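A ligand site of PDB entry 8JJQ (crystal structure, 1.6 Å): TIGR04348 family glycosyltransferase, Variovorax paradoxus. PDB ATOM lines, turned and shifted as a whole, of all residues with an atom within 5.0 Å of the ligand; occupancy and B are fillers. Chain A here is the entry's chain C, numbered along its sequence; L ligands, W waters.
Asn 18 touches the ligand. CA of Gly 84 touches C8 of the ligand (3.3 Å). Leu 110 touches the ligand. Val 151 touches the ligand. CE1 of His 153 touches C11 of the ligand, 3.3 Å away. Val 157 touches the ligand. CG2 of Ile 181 touches O8 of the ligand (3.3 Å). CA of Gly 182 touches O8 of the ligand, at 3.6 Å. CA of Ala 208 touches O8 of the ligand, 3.4 Å away. O of Leu 230 touches O6 of the ligand (3.7 Å). 28 residues have an atom within 4 Å of the ligand: Asn 17, Asn 18, Gly 19, Asn 20, Arg 22, Thr 23, Thr 83, Gly 84, Leu 110, Val 151, His 153, Arg 155, Val 157, Lys 158, Ile 181, Gly 182, Ala 208, Leu 209, His 211, Thr 214, Leu 230, Glu 231, Gly 232, Gly 233, Ala 234, His 235, Val 236 and Glu 239.
The side-chain carboxylate of Glu 231 sits at hydrogen-bond distance from an oxygen (O2) of the ligand. OE2 of Glu 239 is in hydrogen-bond range of O11 of the ligand (2.6 Å). The guanidinium group of Arg 155 lies within salt-bridge range of an oxygen (O17) of the ligand. The backbone carbonyl oxygen of Thr 83 lies within hydrogen-bond range of an oxygen (O3) of the ligand (2.7 Å). OG1 of Thr 23 lies within hydrogen-bond range of O5 of the ligand. N of His 235 sits at hydrogen-bond distance from O14 of the ligand. ND1 of His 235 lies within hydrogen-bond range of O14 of the ligand, 2.9 Å away. O8 of the ligand is in hydrogen-bond range of N of Leu 209 (3.1 Å). A nitrogen (N3) of the ligand is in hydrogen-bond range of the backbone carbonyl oxygen of Leu 209 (2.9 Å). An oxygen (O16) of the ligand is in hydrogen-bond range of the backbone NH (N) of Gly 19 (2.9 Å). O of Gly 19 lies within hydrogen-bond range of O5 of the ligand, at 3.1 Å. The side-chain amino group (NZ) of Lys 158 is in salt-bridge range of an oxygen (O17) of the ligand. An oxygen (O11) of the ligand is in hydrogen-bond range of the guanidinium group of Arg 22 (2.9 Å). N of Gly 233 is in hydrogen-bond range of O2 of the ligand, at 3.0 Å. O2 of the ligand lies within hydrogen-bond range of N of Gly 232. An oxygen (O7) of the ligand is in hydrogen-bond range of the side-chain amide nitrogen of Asn 17 (3.0 Å). An oxygen (O5) of the ligand sits at hydrogen-bond distance from the backbone NH (N) of Asn 20 (3.3 Å). OD1 of Asn 20 sits close to O4 of the ligand, 3.1 Å away. A ring nitrogen (ND1) of His 211 sits close to an oxygen (O7) of the ligand, at 3.2 Å. N3 of the ligand is in hydrogen-bond range of OG1 of Thr 214. The backbone NH (N) of Val 236 sits at hydrogen-bond distance from an oxygen (O13) of the ligand (3.3 Å). N of Ala 234 lies within hydrogen-bond range of O2 of the ligand, 3.5 Å away.
The side-chain carboxylate (OE2) of Glu 231 lies within salt-bridge range of the side-chain amino group (NZ) of Lys 158, 2.8 Å away. The side-chain amide oxygen (OE1) of Gln 131 sits at hydrogen-bond distance from a ring nitrogen (NE2) of His 235 (3.3 Å). O of Leu 209 is in hydrogen-bond range of ND2 of Asn 17. The guanidinium group (NH1) of Arg 22 is in hydrogen-bond range of the side-chain amide oxygen (OD1) of Asn 17 (2.9 Å). The backbone NH (N) of His 211 sits close to the side-chain amide nitrogen (ND2) of Asn 17, 3.3 Å away. A ring nitrogen (NE2) of His 153 lies within hydrogen-bond range of the backbone carbonyl oxygen (O) of Asn 17 (2.8 Å). A ring nitrogen (ND1) of His 153 is in hydrogen-bond range of the backbone NH of Asp 183 (2.9 Å). The backbone NH of Ala 208 sits at hydrogen-bond distance from the backbone carbonyl oxygen of Gly 182 (3.4 Å).
Water W4 lies within hydrogen-bond range of an oxygen (O13) of the ligand, the backbone carbonyl oxygen of Val 151 and the side-chain amino group of Lys 158. Water W2 lies within hydrogen-bond range of an oxygen (O16) of the ligand (2.9 Å), the backbone NH of Asn 20 (3.0 Å) and the backbone NH of Gly 19 (3.4 Å).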
ATOM      1  N   ASN A  17      25.177  16.892  18.947  1.00  0.00           N
ATOM      2  CA  ASN A  17      24.654  15.506  19.106  1.00  0.00           C
ATOM      3  C   ASN A  17      25.842  14.598  18.914  1.00  0.00           C
ATOM      4  O   ASN A  17      26.002  14.035  17.835  1.00  0.00           O
ATOM      5  CB  ASN A  17      23.555  15.226  18.109  1.00  0.00           C
ATOM      6  CG  ASN A  17      22.935  13.859  18.278  1.00  0.00           C
ATOM      7  OD1 ASN A  17      23.135  13.242  19.329  1.00  0.00           O
ATOM      8  ND2 ASN A  17      22.157  13.435  17.291  1.00  0.00           N
ATOM      9  N   ASN A  18      26.672  14.431  19.938  1.00  0.00           N
ATOM     10  CA  ASN A  18      27.844  13.550  19.848  1.00  0.00           C
ATOM     11  C   ASN A  18      28.171  13.024  21.269  1.00  0.00           C
ATOM     12  O   ASN A  18      27.522  13.460  22.221  1.00  0.00           O
ATOM     13  CB  ASN A  18      29.017  14.257  19.138  1.00  0.00           C
ATOM     14  CG  ASN A  18      29.628  15.429  19.891  1.00  0.00           C
ATOM     15  OD1 ASN A  18      29.550  15.528  21.125  1.00  0.00           O
ATOM     16  ND2 ASN A  18      30.132  16.403  19.135  1.00  0.00           N
ATOM     17  N   GLY A  19      29.159  12.150  21.376  1.00  0.00           N
ATOM     18  CA  GLY A  19      29.502  11.515  22.673  1.00  0.00           C
ATOM     19  C   GLY A  19      29.944  12.548  23.657  1.00  0.00           C
ATOM     20  O   GLY A  19      29.540  12.504  24.829  1.00  0.00           O
ATOM     21  N   ASN A  20      30.877  13.408  23.278  1.00  0.00           N
ATOM     22  CA  ASN A  20      31.474  14.300  24.303  1.00  0.00           C
ATOM     23  C   ASN A  20      30.418  15.217  24.921  1.00  0.00           C
ATOM     24  O   ASN A  20      30.501  15.548  26.141  1.00  0.00           O
ATOM     25  CB  ASN A  20      32.570  15.191  23.723  1.00  0.00           C
ATOM     26  CG  ASN A  20      33.826  14.428  23.398  1.00  0.00           C
ATOM     27  OD1 ASN A  20      33.993  13.226  23.707  1.00  0.00           O
ATOM     28  ND2 ASN A  20      34.687  15.081  22.642  1.00  0.00           N
ATOM     29  N   ARG A  22      27.133  14.404  25.112  1.00  0.00           N
ATOM     30  CA  ARG A  22      26.251  13.451  25.793  1.00  0.00           C
ATOM     31  C   ARG A  22      26.821  13.073  27.149  1.00  0.00           C
ATOM     32  O   ARG A  22      26.090  13.168  28.151  1.00  0.00           O
ATOM     33  CB  ARG A  22      25.915  12.265  24.905  1.00  0.00           C
ATOM     34  CG  ARG A  22      24.854  11.337  25.468  1.00  0.00           C
ATOM     35  CD  ARG A  22      23.969  10.731  24.395  1.00  0.00           C
ATOM     36  NE  ARG A  22      23.150  11.808  23.846  1.00  0.00           N
ATOM     37  CZ  ARG A  22      23.225  12.272  22.597  1.00  0.00           C
ATOM     38  NH1 ARG A  22      23.933  11.689  21.652  1.00  0.00           N
ATOM     39  NH2 ARG A  22      22.596  13.399  22.279  1.00  0.00           N
ATOM     40  N   THR A  23      28.094  12.729  27.232  1.00  0.00           N
ATOM     41  CA  THR A  23      28.716  12.344  28.510  1.00  0.00           C
ATOM     42  C   THR A  23      28.578  13.533  29.455  1.00  0.00           C
ATOM     43  O   THR A  23      28.201  13.407  30.633  1.00  0.00           O
ATOM     44  CB  THR A  23      30.198  12.011  28.271  1.00  0.00           C
ATOM     45  OG1 THR A  23      30.349  10.958  27.322  1.00  0.00           O
ATOM     46  CG2 THR A  23      30.871  11.637  29.562  1.00  0.00           C
ATOM     47  N   LEU A  57      37.193  16.406  29.869  1.00  0.00           N
ATOM     48  CA  LEU A  57      37.126  15.366  28.830  1.00  0.00           C
ATOM     49  C   LEU A  57      38.167  15.671  27.759  1.00  0.00           C
ATOM     50  O   LEU A  57      38.147  16.813  27.188  1.00  0.00           O
ATOM     51  CB  LEU A  57      35.726  15.384  28.218  1.00  0.00           C
ATOM     52  CG  LEU A  57      34.687  14.531  28.935  1.00  0.00           C
ATOM     53  CD1 LEU A  57      34.450  15.018  30.358  1.00  0.00           C
ATOM     54  CD2 LEU A  57      33.385  14.476  28.117  1.00  0.00           C
ATOM     55  N   THR A  83      38.835   9.983  26.571  1.00  0.00           N
ATOM     56  CA  THR A  83      37.608   9.757  25.765  1.00  0.00           C
ATOM     57  C   THR A  83      37.933   9.038  24.450  1.00  0.00           C
ATOM     58  O   THR A  83      36.979   8.584  23.790  1.00  0.00           O
ATOM     59  CB  THR A  83      36.810  11.026  25.534  1.00  0.00           C
ATOM     60  OG1 THR A  83      37.671  11.952  24.882  1.00  0.00           O
ATOM     61  CG2 THR A  83      36.208  11.639  26.776  1.00  0.00           C
ATOM     62  N   GLY A  84      39.188   8.822  24.063  1.00  0.00           N
ATOM     63  CA  GLY A  84      39.416   8.003  22.857  1.00  0.00           C
ATOM     64  C   GLY A  84      40.771   8.254  22.215  1.00  0.00           C
ATOM     65  O   GLY A  84      41.685   7.475  22.485  1.00  0.00           O
ATOM     66  N   THR A  85      40.889   9.246  21.330  1.00  0.00           N
ATOM     67  CA  THR A  85      42.122   9.524  20.558  1.00  0.00           C
ATOM     68  C   THR A  85      43.259   9.984  21.471  1.00  0.00           C
ATOM     69  O   THR A  85      44.417   9.868  21.072  1.00  0.00           O
ATOM     70  CB  THR A  85      41.868  10.531  19.417  1.00  0.00           C
ATOM     71  OG1 THR A  85      41.455  11.780  19.956  1.00  0.00           O
ATOM     72  CG2 THR A  85      40.775  10.044  18.492  1.00  0.00           C
ATOM     73  N   LEU A 110      36.714   4.692  30.394  1.00  0.00           N
ATOM     74  CA  LEU A 110      35.249   4.463  30.248  1.00  0.00           C
ATOM     75  C   LEU A 110      34.935   2.989  30.015  1.00  0.00           C
ATOM     76  O   LEU A 110      33.746   2.647  29.771  1.00  0.00           O
ATOM     77  CB  LEU A 110      34.744   5.335  29.104  1.00  0.00           C
ATOM     78  CG  LEU A 110      34.965   6.854  29.222  1.00  0.00           C
ATOM     79  CD1 LEU A 110      34.477   7.606  27.989  1.00  0.00           C
ATOM     80  CD2 LEU A 110      34.318   7.443  30.448  1.00  0.00           C
ATOM     81  N   GLN A 131      30.071   4.041  30.998  1.00  0.00           N
ATOM     82  CA  GLN A 131      28.948   4.965  30.720  1.00  0.00           C
ATOM     83  C   GLN A 131      27.639   4.216  30.867  1.00  0.00           C
ATOM     84  O   GLN A 131      27.593   2.988  31.039  1.00  0.00           O
ATOM     85  CB  GLN A 131      29.106   5.650  29.389  1.00  0.00           C
ATOM     86  CG  GLN A 131      30.476   6.339  29.247  1.00  0.00           C
ATOM     87  CD  GLN A 131      30.504   7.233  28.040  1.00  0.00           C
ATOM     88  OE1 GLN A 131      30.146   8.385  28.119  1.00  0.00           O
ATOM     89  NE2 GLN A 131      30.808   6.664  26.871  1.00  0.00           N
ATOM     90  N   VAL A 151      26.132   3.573  13.430  1.00  0.00           N
ATOM     91  CA  VAL A 151      25.913   4.948  13.855  1.00  0.00           C
ATOM     92  C   VAL A 151      27.252   5.593  14.201  1.00  0.00           C
ATOM     93  O   VAL A 151      27.910   5.191  15.115  1.00  0.00           O
ATOM     94  CB  VAL A 151      24.910   5.010  15.019  1.00  0.00           C
ATOM     95  CG1 VAL A 151      24.695   6.442  15.492  1.00  0.00           C
ATOM     96  CG2 VAL A 151      23.590   4.300  14.693  1.00  0.00           C
ATOM     97  N   GLY A 152      27.576   6.662  13.510  1.00  0.00           N
ATOM     98  CA  GLY A 152      28.728   7.496  13.829  1.00  0.00           C
ATOM     99  C   GLY A 152      28.921   8.580  12.825  1.00  0.00           C
ATOM    100  O   GLY A 152      28.963   8.244  11.634  1.00  0.00           O
ATOM    101  N   HIS A 153      29.140   9.811  13.269  1.00  0.00           N
ATOM    102  CA  HIS A 153      29.522  10.921  12.381  1.00  0.00           C
ATOM    103  C   HIS A 153      30.765  10.452  11.633  1.00  0.00           C
ATOM    104  O   HIS A 153      31.704   9.892  12.273  1.00  0.00           O
ATOM    105  CB  HIS A 153      29.647  12.206  13.185  1.00  0.00           C
ATOM    106  CG  HIS A 153      28.393  12.668  13.833  1.00  0.00           C
ATOM    107  ND1 HIS A 153      27.218  12.869  13.116  1.00  0.00           N
ATOM    108  CD2 HIS A 153      28.105  12.934  15.128  1.00  0.00           C
ATOM    109  CE1 HIS A 153      26.287  13.295  13.948  1.00  0.00           C
ATOM    110  NE2 HIS A 153      26.812  13.383  15.186  1.00  0.00           N
ATOM    111  N   ARG A 155      34.046   9.999  10.263  1.00  0.00           N
ATOM    112  CA  ARG A 155      35.441  10.429  10.425  1.00  0.00           C
ATOM    113  C   ARG A 155      36.343   9.209  10.360  1.00  0.00           C
ATOM    114  O   ARG A 155      35.888   8.060  10.575  1.00  0.00           O
ATOM    115  CB  ARG A 155      35.728  11.213  11.718  1.00  0.00           C
ATOM    116  CG  ARG A 155      34.908  10.867  12.930  1.00  0.00           C
ATOM    117  CD  ARG A 155      35.637  11.404  14.158  1.00  0.00           C
ATOM    118  NE  ARG A 155      34.977  11.030  15.392  1.00  0.00           N
ATOM    119  CZ  ARG A 155      35.403  11.351  16.590  1.00  0.00           C
ATOM    120  NH1 ARG A 155      36.514  12.051  16.727  1.00  0.00           N
ATOM    121  NH2 ARG A 155      34.721  10.964  17.662  1.00  0.00           N
ATOM    122  N   VAL A 157      38.463   7.782  12.197  1.00  0.00           N
ATOM    123  CA  VAL A 157      38.606   6.956  13.430  1.00  0.00           C
ATOM    124  C   VAL A 157      37.457   5.938  13.491  1.00  0.00           C
ATOM    125  O   VAL A 157      37.601   4.875  14.151  1.00  0.00           O
ATOM    126  CB  VAL A 157      38.672   7.828  14.695  1.00  0.00           C
ATOM    127  CG1 VAL A 157      37.384   8.584  14.969  1.00  0.00           C
ATOM    128  CG2 VAL A 157      39.094   6.959  15.843  1.00  0.00           C
ATOM    129  N   LYS A 158      36.321   6.250  12.817  1.00  0.00           N
ATOM    130  CA  LYS A 158      35.178   5.311  12.756  1.00  0.00           C
ATOM    131  C   LYS A 158      35.347   4.235  11.681  1.00  0.00           C
ATOM    132  O   LYS A 158      34.558   3.290  11.685  1.00  0.00           O
ATOM    133  CB  LYS A 158      33.842   6.035  12.507  1.00  0.00           C
ATOM    134  CG  LYS A 158      33.521   7.090  13.549  1.00  0.00           C
ATOM    135  CD  LYS A 158      33.075   6.451  14.899  1.00  0.00           C
ATOM    136  CE  LYS A 158      32.869   7.513  15.964  1.00  0.00           C
ATOM    137  NZ  LYS A 158      32.420   6.951  17.246  1.00  0.00           N
ATOM    138  N   ILE A 181      24.051   5.942   9.792  1.00  0.00           N
ATOM    139  CA  ILE A 181      23.622   7.227  10.360  1.00  0.00           C
ATOM    140  C   ILE A 181      24.882   7.976  10.788  1.00  0.00           C
ATOM    141  O   ILE A 181      25.730   7.369  11.505  1.00  0.00           O
ATOM    142  CB  ILE A 181      22.662   6.994  11.560  1.00  0.00           C
ATOM    143  CG1 ILE A 181      21.383   6.246  11.119  1.00  0.00           C
ATOM    144  CG2 ILE A 181      22.353   8.326  12.214  1.00  0.00           C
ATOM    145  CD1 ILE A 181      20.553   5.671  12.285  1.00  0.00           C
ATOM    146  N   GLY A 182      24.975   9.253  10.438  1.00  0.00           N
ATOM    147  CA  GLY A 182      26.075  10.156  10.827  1.00  0.00           C
ATOM    148  C   GLY A 182      26.338  11.257   9.802  1.00  0.00           C
ATOM    149  O   GLY A 182      26.072  11.049   8.596  1.00  0.00           O
ATOM    150  N   ASP A 183      26.801  12.376  10.287  1.00  0.00           N
ATOM    151  CA  ASP A 183      27.115  13.541   9.410  1.00  0.00           C
ATOM    152  C   ASP A 183      28.291  13.206   8.472  1.00  0.00           C
ATOM    153  O   ASP A 183      29.045  12.285   8.732  1.00  0.00           O
ATOM    154  CB  ASP A 183      27.523  14.755  10.248  1.00  0.00           C
ATOM    155  CG  ASP A 183      27.395  16.093   9.542  1.00  0.00           C
ATOM    156  OD1 ASP A 183      26.309  16.342   8.987  1.00  0.00           O
ATOM    157  OD2 ASP A 183      28.381  16.867   9.592  1.00  0.00           O
ATOM    158  N   GLY A 207      22.609  10.253   6.618  1.00  0.00           N
ATOM    159  CA  GLY A 207      23.118  11.525   7.148  1.00  0.00           C
ATOM    160  C   GLY A 207      22.949  11.547   8.639  1.00  0.00           C
ATOM    161  O   GLY A 207      22.636  10.496   9.226  1.00  0.00           O
ATOM    162  N   ALA A 208      23.126  12.702   9.250  1.00  0.00           N
ATOM    163  CA  ALA A 208      22.973  12.873  10.711  1.00  0.00           C
ATOM    164  C   ALA A 208      21.484  12.858  11.049  1.00  0.00           C
ATOM    165  O   ALA A 208      20.689  13.486  10.344  1.00  0.00           O
ATOM    166  CB  ALA A 208      23.641  14.140  11.130  1.00  0.00           C
ATOM    167  N   LEU A 209      21.104  12.203  12.135  1.00  0.00           N
ATOM    168  CA  LEU A 209      19.710  12.152  12.585  1.00  0.00           C
ATOM    169  C   LEU A 209      19.724  12.587  14.036  1.00  0.00           C
ATOM    170  O   LEU A 209      20.631  12.326  14.834  1.00  0.00           O
ATOM    171  CB  LEU A 209      19.109  10.756  12.437  1.00  0.00           C
ATOM    172  CG  LEU A 209      18.951  10.245  10.992  1.00  0.00           C
ATOM    173  CD1 LEU A 209      18.456   8.801  10.963  1.00  0.00           C
ATOM    174  CD2 LEU A 209      18.078  11.197  10.208  1.00  0.00           C
ATOM    175  N   PRO A 210      18.572  13.159  14.440  1.00  0.00           N
ATOM    176  CA  PRO A 210      18.461  13.477  15.855  1.00  0.00           C
ATOM    177  C   PRO A 210      18.588  12.212  16.719  1.00  0.00           C
ATOM    178  O   PRO A 210      18.216  11.076  16.298  1.00  0.00           O
ATOM    179  CB  PRO A 210      17.042  13.996  15.982  1.00  0.00           C
ATOM    180  CG  PRO A 210      16.661  14.421  14.572  1.00  0.00           C
ATOM    181  CD  PRO A 210      17.365  13.451  13.635  1.00  0.00           C
ATOM    182  N   HIS A 211      19.059  12.404  17.929  1.00  0.00           N
ATOM    183  CA  HIS A 211      19.262  11.276  18.881  1.00  0.00           C
ATOM    184  C   HIS A 211      17.982  10.442  19.129  1.00  0.00           C
ATOM    185  O   HIS A 211      18.081   9.226  19.196  1.00  0.00           O
ATOM    186  CB  HIS A 211      19.871  11.810  20.161  1.00  0.00           C
ATOM    187  CG  HIS A 211      20.314  10.754  21.084  1.00  0.00           C
ATOM    188  ND1 HIS A 211      21.238   9.776  20.699  1.00  0.00           N
ATOM    189  CD2 HIS A 211      19.892  10.395  22.310  1.00  0.00           C
ATOM    190  CE1 HIS A 211      21.359   8.915  21.701  1.00  0.00           C
ATOM    191  NE2 HIS A 211      20.661   9.354  22.719  1.00  0.00           N
ATOM    192  N   THR A 214      17.584   8.221  16.190  1.00  0.00           N
ATOM    193  CA  THR A 214      18.750   7.298  16.169  1.00  0.00           C
ATOM    194  C   THR A 214      18.501   6.138  17.158  1.00  0.00           C
ATOM    195  O   THR A 214      18.652   4.967  16.796  1.00  0.00           O
ATOM    196  CB  THR A 214      20.034   8.114  16.384  1.00  0.00           C
ATOM    197  OG1 THR A 214      20.126   9.084  15.340  1.00  0.00           O
ATOM    198  CG2 THR A 214      21.258   7.244  16.379  1.00  0.00           C
ATOM    199  N   ILE A 218      18.140   2.186  16.176  1.00  0.00           N
ATOM    200  CA  ILE A 218      18.998   1.138  16.815  1.00  0.00           C
ATOM    201  C   ILE A 218      18.101   0.022  17.384  1.00  0.00           C
ATOM    202  O   ILE A 218      18.411  -1.171  17.234  1.00  0.00           O
ATOM    203  CB  ILE A 218      19.919   1.769  17.863  1.00  0.00           C
ATOM    204  CG1 ILE A 218      21.039   2.606  17.240  1.00  0.00           C
ATOM    205  CG2 ILE A 218      20.494   0.687  18.755  1.00  0.00           C
ATOM    206  CD1 ILE A 218      21.805   3.492  18.196  1.00  0.00           C
ATOM    207  N   LEU A 230      39.408   2.806  17.006  1.00  0.00           N
ATOM    208  CA  LEU A 230      39.562   3.005  18.461  1.00  0.00           C
ATOM    209  C   LEU A 230      38.251   3.586  18.951  1.00  0.00           C
ATOM    210  O   LEU A 230      37.628   4.381  18.212  1.00  0.00           O
ATOM    211  CB  LEU A 230      40.767   3.911  18.748  1.00  0.00           C
ATOM    212  CG  LEU A 230      40.661   5.348  18.240  1.00  0.00           C
ATOM    213  CD1 LEU A 230      40.110   6.308  19.284  1.00  0.00           C
ATOM    214  CD2 LEU A 230      42.014   5.873  17.739  1.00  0.00           C
ATOM    215  N   GLU A 231      37.994   3.350  20.236  1.00  0.00           N
ATOM    216  CA  GLU A 231      36.910   4.040  20.973  1.00  0.00           C
ATOM    217  C   GLU A 231      37.353   4.204  22.442  1.00  0.00           C
ATOM    218  O   GLU A 231      37.915   3.239  22.970  1.00  0.00           O
ATOM    219  CB  GLU A 231      35.635   3.173  20.949  1.00  0.00           C
ATOM    220  CG  GLU A 231      34.927   3.189  19.561  1.00  0.00           C
ATOM    221  CD  GLU A 231      34.256   4.481  19.140  1.00  0.00           C
ATOM    222  OE1 GLU A 231      34.037   5.397  19.972  1.00  0.00           O
ATOM    223  OE2 GLU A 231      33.867   4.609  17.918  1.00  0.00           O
ATOM    224  N   GLY A 232      36.958   5.300  23.098  1.00  0.00           N
ATOM    225  CA  GLY A 232      37.083   5.384  24.575  1.00  0.00           C
ATOM    226  C   GLY A 232      36.096   4.429  25.226  1.00  0.00           C
ATOM    227  O   GLY A 232      36.403   3.783  26.249  1.00  0.00           O
ATOM    228  N   GLY A 233      34.896   4.302  24.651  1.00  0.00           N
ATOM    229  CA  GLY A 233      33.785   3.460  25.163  1.00  0.00           C
ATOM    230  C   GLY A 233      32.509   3.952  24.551  1.00  0.00           C
ATOM    231  O   GLY A 233      31.875   4.837  25.112  1.00  0.00           O
ATOM    232  N   ALA A 234      32.174   3.450  23.381  1.00  0.00           N
ATOM    233  CA  ALA A 234      31.184   4.068  22.467  1.00  0.00           C
ATOM    234  C   ALA A 234      29.760   4.036  22.981  1.00  0.00           C
ATOM    235  O   ALA A 234      29.281   2.917  23.373  1.00  0.00           O
ATOM    236  CB  ALA A 234      31.199   3.377  21.128  1.00  0.00           C
ATOM    237  N   HIS A 235      29.070   5.191  22.970  1.00  0.00           N
ATOM    238  CA  HIS A 235      27.636   5.277  23.368  1.00  0.00           C
ATOM    239  C   HIS A 235      26.837   4.337  22.487  1.00  0.00           C
ATOM    240  O   HIS A 235      25.896   3.722  22.980  1.00  0.00           O
ATOM    241  CB  HIS A 235      27.068   6.699  23.244  1.00  0.00           C
ATOM    242  CG  HIS A 235      27.486   7.657  24.313  1.00  0.00           C
ATOM    243  ND1 HIS A 235      28.605   8.382  24.157  1.00  0.00           N
ATOM    244  CD2 HIS A 235      26.869   8.157  25.425  1.00  0.00           C
ATOM    245  CE1 HIS A 235      28.710   9.271  25.169  1.00  0.00           C
ATOM    246  NE2 HIS A 235      27.676   9.065  25.973  1.00  0.00           N
ATOM    247  N   VAL A 236      27.117   4.277  21.181  1.00  0.00           N
ATOM    248  CA  VAL A 236      26.198   3.525  20.302  1.00  0.00           C
ATOM    249  C   VAL A 236      26.215   2.054  20.657  1.00  0.00           C
ATOM    250  O   VAL A 236      25.117   1.414  20.516  1.00  0.00           O
ATOM    251  CB  VAL A 236      26.495   3.772  18.814  1.00  0.00           C
ATOM    252  CG1 VAL A 236      26.215   5.225  18.470  1.00  0.00           C
ATOM    253  CG2 VAL A 236      27.890   3.307  18.421  1.00  0.00           C
ATOM    254  N   GLU A 239      23.849   1.771  23.633  1.00  0.00           N
ATOM    255  CA  GLU A 239      22.495   2.054  23.146  1.00  0.00           C
ATOM    256  C   GLU A 239      21.906   0.793  22.510  1.00  0.00           C
ATOM    257  O   GLU A 239      20.747   0.419  22.810  1.00  0.00           O
ATOM    258  CB  GLU A 239      22.524   3.253  22.218  1.00  0.00           C
ATOM    259  CG  GLU A 239      22.903   4.518  22.984  1.00  0.00           C
ATOM    260  CD  GLU A 239      23.279   5.715  22.124  1.00  0.00           C
ATOM    261  OE1 GLU A 239      23.329   5.584  20.865  1.00  0.00           O
ATOM    262  OE2 GLU A 239      23.578   6.778  22.695  1.00  0.00           O
HETATM  263  C1  LIG L   1      33.608   9.800  21.754  1.00  0.00           C
HETATM  264  C2  LIG L   1      34.403   8.501  21.719  1.00  0.00           C
HETATM  265  C3  LIG L   1      33.590   7.443  22.477  1.00  0.00           C
HETATM  266  C4  LIG L   1      33.347   7.882  23.910  1.00  0.00           C
HETATM  267  C5  LIG L   1      32.797   9.314  23.940  1.00  0.00           C
HETATM  268  C6  LIG L   1      32.876   9.921  25.340  1.00  0.00           C
HETATM  269  C7  LIG L   1      35.896   7.841  19.808  1.00  0.00           C
HETATM  270  C8  LIG L   1      36.931   7.440  20.795  1.00  0.00           C
HETATM  271  N1  LIG L   1      34.698   8.203  20.329  1.00  0.00           N
HETATM  272  O1  LIG L   1      32.310   9.644  21.138  1.00  0.00           O
HETATM  273  O2  LIG L   1      34.158   6.121  22.432  1.00  0.00           O
HETATM  274  O3  LIG L   1      34.546   7.771  24.660  1.00  0.00           O
HETATM  275  O4  LIG L   1      33.471  10.258  23.071  1.00  0.00           O
HETATM  276  O5  LIG L   1      32.273  11.210  25.351  1.00  0.00           O
HETATM  277  O6  LIG L   1      36.146   7.719  18.589  1.00  0.00           O
HETATM  278  N2  LIG L   1      24.314  10.113  17.309  1.00  0.00           N
HETATM  279  C9  LIG L   1      23.034  10.432  16.902  1.00  0.00           C
HETATM  280  N3  LIG L   1      22.904  10.753  15.563  1.00  0.00           N
HETATM  281  C10 LIG L   1      23.942  10.785  14.626  1.00  0.00           C
HETATM  282  C11 LIG L   1      25.234  10.405  15.128  1.00  0.00           C
HETATM  283  C12 LIG L   1      25.378  10.043  16.417  1.00  0.00           C
HETATM  284  O7  LIG L   1      22.090  10.466  17.688  1.00  0.00           O
HETATM  285  O8  LIG L   1      23.706  11.065  13.441  1.00  0.00           O
HETATM  286  C13 LIG L   1      24.514   9.865  18.736  1.00  0.00           C
HETATM  287  C14 LIG L   1      24.683   8.409  19.173  1.00  0.00           C
HETATM  288  O9  LIG L   1      23.385   7.857  19.263  1.00  0.00           O
HETATM  289  C15 LIG L   1      25.504   8.590  20.463  1.00  0.00           C
HETATM  290  C16 LIG L   1      26.402   9.766  20.087  1.00  0.00           C
HETATM  291  O10 LIG L   1      25.701  10.533  19.080  1.00  0.00           O
HETATM  292  O11 LIG L   1      24.656   8.880  21.558  1.00  0.00           O
HETATM  293  C17 LIG L   1      27.793   9.389  19.590  1.00  0.00           C
HETATM  294  O12 LIG L   1      28.577   8.921  20.719  1.00  0.00           O
HETATM  295  P1  LIG L   1      29.683   7.763  20.589  1.00  0.00           P
HETATM  296  O13 LIG L   1      29.127   6.556  19.878  1.00  0.00           O
HETATM  297  O14 LIG L   1      30.224   7.549  21.953  1.00  0.00           O
HETATM  298  O15 LIG L   1      30.847   8.354  19.675  1.00  0.00           O
HETATM  299  P2  LIG L   1      31.725   9.707  19.667  1.00  0.00           P
HETATM  300  O16 LIG L   1      30.935  10.935  19.484  1.00  0.00           O
HETATM  301  O17 LIG L   1      32.818   9.410  18.705  1.00  0.00           O
HETATM  302  O   HOH W   1      30.805  11.691  16.875  1.00  0.00           O
HETATM  303  O   HOH W   2      32.237  13.276  20.643  1.00  0.00           O
HETATM  304  O   HOH W   3      29.036   9.618  16.338  1.00  0.00           O
HETATM  305  O   HOH W   4      29.485   6.652  17.078  1.00  0.00           O
